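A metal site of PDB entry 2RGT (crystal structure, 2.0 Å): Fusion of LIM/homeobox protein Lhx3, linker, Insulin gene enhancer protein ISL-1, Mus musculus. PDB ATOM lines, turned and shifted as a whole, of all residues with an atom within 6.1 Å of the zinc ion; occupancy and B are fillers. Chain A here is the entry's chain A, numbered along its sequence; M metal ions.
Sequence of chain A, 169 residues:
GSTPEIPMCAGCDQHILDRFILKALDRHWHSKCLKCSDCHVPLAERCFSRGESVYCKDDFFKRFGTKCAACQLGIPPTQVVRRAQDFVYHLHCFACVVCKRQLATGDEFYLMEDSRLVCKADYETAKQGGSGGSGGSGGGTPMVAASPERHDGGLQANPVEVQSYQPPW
The zinc ion is bound by a ring nitrogen (ND1) of His 30 (2.0 Å).
The zinc ion is bound by SG of Cys 9 (2.1 Å).
SG of Cys 33 is bound to the zinc ion (2.3 Å).
The zinc ion is bound by the side-chain sulfur (SG) of Cys 12 (2.6 Å).
The zinc ion has four donor atoms within binding distance.
The backbone NH (N) of Cys 9 lies within hydrogen-bond range of the backbone carbonyl oxygen (O) of Gln 14 (3.3 Å).
The side-chain sulfur (SG) of Cys 12 lies close to the backbone NH (N) of Gln 14 (3.7 Å).
N of Gly 11 lies close to SG of Cys 9 (3.5 Å).
NE2 of His 30 sits at hydrogen-bond distance from O of His 15 (3.2 Å).
Of the 12 residues printed, 4 come within 4 Å of the zinc ion.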
ATOM      1  N   CYS A   9     -16.644 -12.673   8.061  1.00  0.00           N
ATOM      2  CA  CYS A   9     -18.010 -12.951   7.618  1.00  0.00           C
ATOM      3  C   CYS A   9     -18.867 -11.745   8.004  1.00  0.00           C
ATOM      4  O   CYS A   9     -18.672 -11.151   9.060  1.00  0.00           O
ATOM      5  CB  CYS A   9     -18.482 -14.312   8.130  1.00  0.00           C
ATOM      6  SG  CYS A   9     -20.214 -14.366   8.638  1.00  0.00           S
ATOM      7  N   ALA A  10     -19.678 -11.306   7.046  1.00  0.00           N
ATOM      8  CA  ALA A  10     -20.116  -9.918   7.111  1.00  0.00           C
ATOM      9  C   ALA A  10     -21.401 -10.041   7.900  1.00  0.00           C
ATOM     10  O   ALA A  10     -22.092  -9.063   8.192  1.00  0.00           O
ATOM     11  CB  ALA A  10     -20.400  -9.383   5.712  1.00  0.00           C
ATOM     12  N   GLY A  11     -21.736 -11.278   8.238  1.00  0.00           N
ATOM     13  CA  GLY A  11     -22.958 -11.566   8.967  1.00  0.00           C
ATOM     14  C   GLY A  11     -22.787 -11.413  10.458  1.00  0.00           C
ATOM     15  O   GLY A  11     -23.606 -10.779  11.136  1.00  0.00           O
ATOM     16  N   CYS A  12     -21.732 -12.052  10.960  1.00  0.00           N
ATOM     17  CA  CYS A  12     -21.400 -12.110  12.354  1.00  0.00           C
ATOM     18  C   CYS A  12     -19.915 -11.973  12.349  1.00  0.00           C
ATOM     19  O   CYS A  12     -19.202 -12.872  11.907  1.00  0.00           O
ATOM     20  CB  CYS A  12     -21.708 -13.487  12.911  1.00  0.00           C
ATOM     21  SG  CYS A  12     -20.357 -14.673  12.738  1.00  0.00           S
ATOM     22  N   ASP A  13     -19.420 -10.832  12.794  1.00  0.00           N
ATOM     23  CA  ASP A  13     -18.027 -10.558  12.554  1.00  0.00           C
ATOM     24  C   ASP A  13     -16.950 -11.579  12.917  1.00  0.00           C
ATOM     25  O   ASP A  13     -15.772 -11.386  12.658  1.00  0.00           O
ATOM     26  CB  ASP A  13     -17.767  -9.054  12.642  1.00  0.00           C
ATOM     27  CG  ASP A  13     -18.652  -8.261  11.686  1.00  0.00           C
ATOM     28  OD1 ASP A  13     -18.585  -8.513  10.477  1.00  0.00           O
ATOM     29  OD2 ASP A  13     -19.405  -7.401  12.159  1.00  0.00           O
ATOM     30  N   GLN A  14     -17.391 -12.688  13.518  1.00  0.00           N
ATOM     31  CA  GLN A  14     -16.334 -13.682  13.462  1.00  0.00           C
ATOM     32  C   GLN A  14     -15.893 -13.968  12.025  1.00  0.00           C
ATOM     33  O   GLN A  14     -16.710 -14.042  11.116  1.00  0.00           O
ATOM     34  CB  GLN A  14     -16.767 -14.974  14.140  1.00  0.00           C
ATOM     35  CG  GLN A  14     -17.380 -14.773  15.519  1.00  0.00           C
ATOM     36  CD  GLN A  14     -17.284 -16.010  16.393  1.00  0.00           C
ATOM     37  OE1 GLN A  14     -16.540 -16.945  16.076  1.00  0.00           O
ATOM     38  NE2 GLN A  14     -18.028 -16.025  17.493  1.00  0.00           N
ATOM     39  N   HIS A  15     -14.582 -14.144  11.846  1.00  0.00           N
ATOM     40  CA  HIS A  15     -14.019 -14.725  10.615  1.00  0.00           C
ATOM     41  C   HIS A  15     -14.463 -16.161  10.353  1.00  0.00           C
ATOM     42  O   HIS A  15     -15.113 -16.780  11.206  1.00  0.00           O
ATOM     43  CB  HIS A  15     -12.494 -14.628  10.627  1.00  0.00           C
ATOM     44  CG  HIS A  15     -11.971 -13.244  10.811  1.00  0.00           C
ATOM     45  ND1 HIS A  15     -11.976 -12.589  12.025  1.00  0.00           N
ATOM     46  CD2 HIS A  15     -11.421 -12.374   9.921  1.00  0.00           C
ATOM     47  CE1 HIS A  15     -11.454 -11.391  11.886  1.00  0.00           C
ATOM     48  NE2 HIS A  15     -11.115 -11.225  10.618  1.00  0.00           N
ATOM     49  N   ILE A  16     -14.113 -16.704   9.185  1.00  0.00           N
ATOM     50  CA  ILE A  16     -14.775 -17.947   8.669  1.00  0.00           C
ATOM     51  C   ILE A  16     -13.822 -19.128   8.450  1.00  0.00           C
ATOM     52  O   ILE A  16     -12.986 -19.090   7.547  1.00  0.00           O
ATOM     53  CB  ILE A  16     -15.573 -17.713   7.353  1.00  0.00           C
ATOM     54  CG1 ILE A  16     -16.376 -16.415   7.412  1.00  0.00           C
ATOM     55  CG2 ILE A  16     -16.493 -18.889   7.050  1.00  0.00           C
ATOM     56  CD1 ILE A  16     -16.672 -15.848   6.053  1.00  0.00           C
ATOM     57  N   TRP A  29     -19.335 -15.075   3.883  1.00  0.00           N
ATOM     58  CA  TRP A  29     -20.320 -15.462   4.894  1.00  0.00           C
ATOM     59  C   TRP A  29     -20.111 -16.915   5.362  1.00  0.00           C
ATOM     60  O   TRP A  29     -19.851 -17.802   4.533  1.00  0.00           O
ATOM     61  CB  TRP A  29     -21.763 -15.361   4.314  1.00  0.00           C
ATOM     62  CG  TRP A  29     -22.112 -14.061   3.645  1.00  0.00           C
ATOM     63  CD1 TRP A  29     -21.779 -13.660   2.364  1.00  0.00           C
ATOM     64  CD2 TRP A  29     -22.870 -12.984   4.208  1.00  0.00           C
ATOM     65  NE1 TRP A  29     -22.271 -12.400   2.123  1.00  0.00           N
ATOM     66  CE2 TRP A  29     -22.927 -11.954   3.231  1.00  0.00           C
ATOM     67  CE3 TRP A  29     -23.494 -12.791   5.452  1.00  0.00           C
ATOM     68  CZ2 TRP A  29     -23.629 -10.750   3.454  1.00  0.00           C
ATOM     69  CZ3 TRP A  29     -24.171 -11.578   5.686  1.00  0.00           C
ATOM     70  CH2 TRP A  29     -24.244 -10.581   4.680  1.00  0.00           C
ATOM     71  N   HIS A  30     -20.277 -17.157   6.668  1.00  0.00           N
ATOM     72  CA  HIS A  30     -20.716 -18.489   7.137  1.00  0.00           C
ATOM     73  C   HIS A  30     -22.076 -18.687   6.487  1.00  0.00           C
ATOM     74  O   HIS A  30     -22.825 -17.730   6.357  1.00  0.00           O
ATOM     75  CB  HIS A  30     -20.983 -18.518   8.643  1.00  0.00           C
ATOM     76  CG  HIS A  30     -19.789 -18.237   9.488  1.00  0.00           C
ATOM     77  ND1 HIS A  30     -19.648 -17.069  10.211  1.00  0.00           N
ATOM     78  CD2 HIS A  30     -18.666 -18.962   9.724  1.00  0.00           C
ATOM     79  CE1 HIS A  30     -18.497 -17.083  10.847  1.00  0.00           C
ATOM     80  NE2 HIS A  30     -17.877 -18.222  10.571  1.00  0.00           N
ATOM     81  N   LYS A  32     -24.626 -20.199   7.832  1.00  0.00           N
ATOM     82  CA  LYS A  32     -25.565 -19.935   8.921  1.00  0.00           C
ATOM     83  C   LYS A  32     -25.926 -18.434   9.012  1.00  0.00           C
ATOM     84  O   LYS A  32     -27.033 -18.067   9.439  1.00  0.00           O
ATOM     85  CB  LYS A  32     -24.964 -20.421  10.263  1.00  0.00           C
ATOM     86  CG  LYS A  32     -24.369 -21.881  10.253  1.00  0.00           C
ATOM     87  CD  LYS A  32     -25.409 -22.908   9.730  1.00  0.00           C
ATOM     88  CE  LYS A  32     -25.143 -24.373  10.115  1.00  0.00           C
ATOM     89  NZ  LYS A  32     -26.159 -25.294   9.452  1.00  0.00           N
ATOM     90  N   CYS A  33     -24.984 -17.585   8.544  1.00  0.00           N
ATOM     91  CA  CYS A  33     -25.063 -16.116   8.616  1.00  0.00           C
ATOM     92  C   CYS A  33     -25.584 -15.383   7.387  1.00  0.00           C
ATOM     93  O   CYS A  33     -25.943 -14.191   7.489  1.00  0.00           O
ATOM     94  CB  CYS A  33     -23.682 -15.558   8.923  1.00  0.00           C
ATOM     95  SG  CYS A  33     -23.133 -16.067  10.510  1.00  0.00           S
HETATM   96 ZN    ZN M   1     -20.876 -15.509  10.296  1.00  0.00          ZN
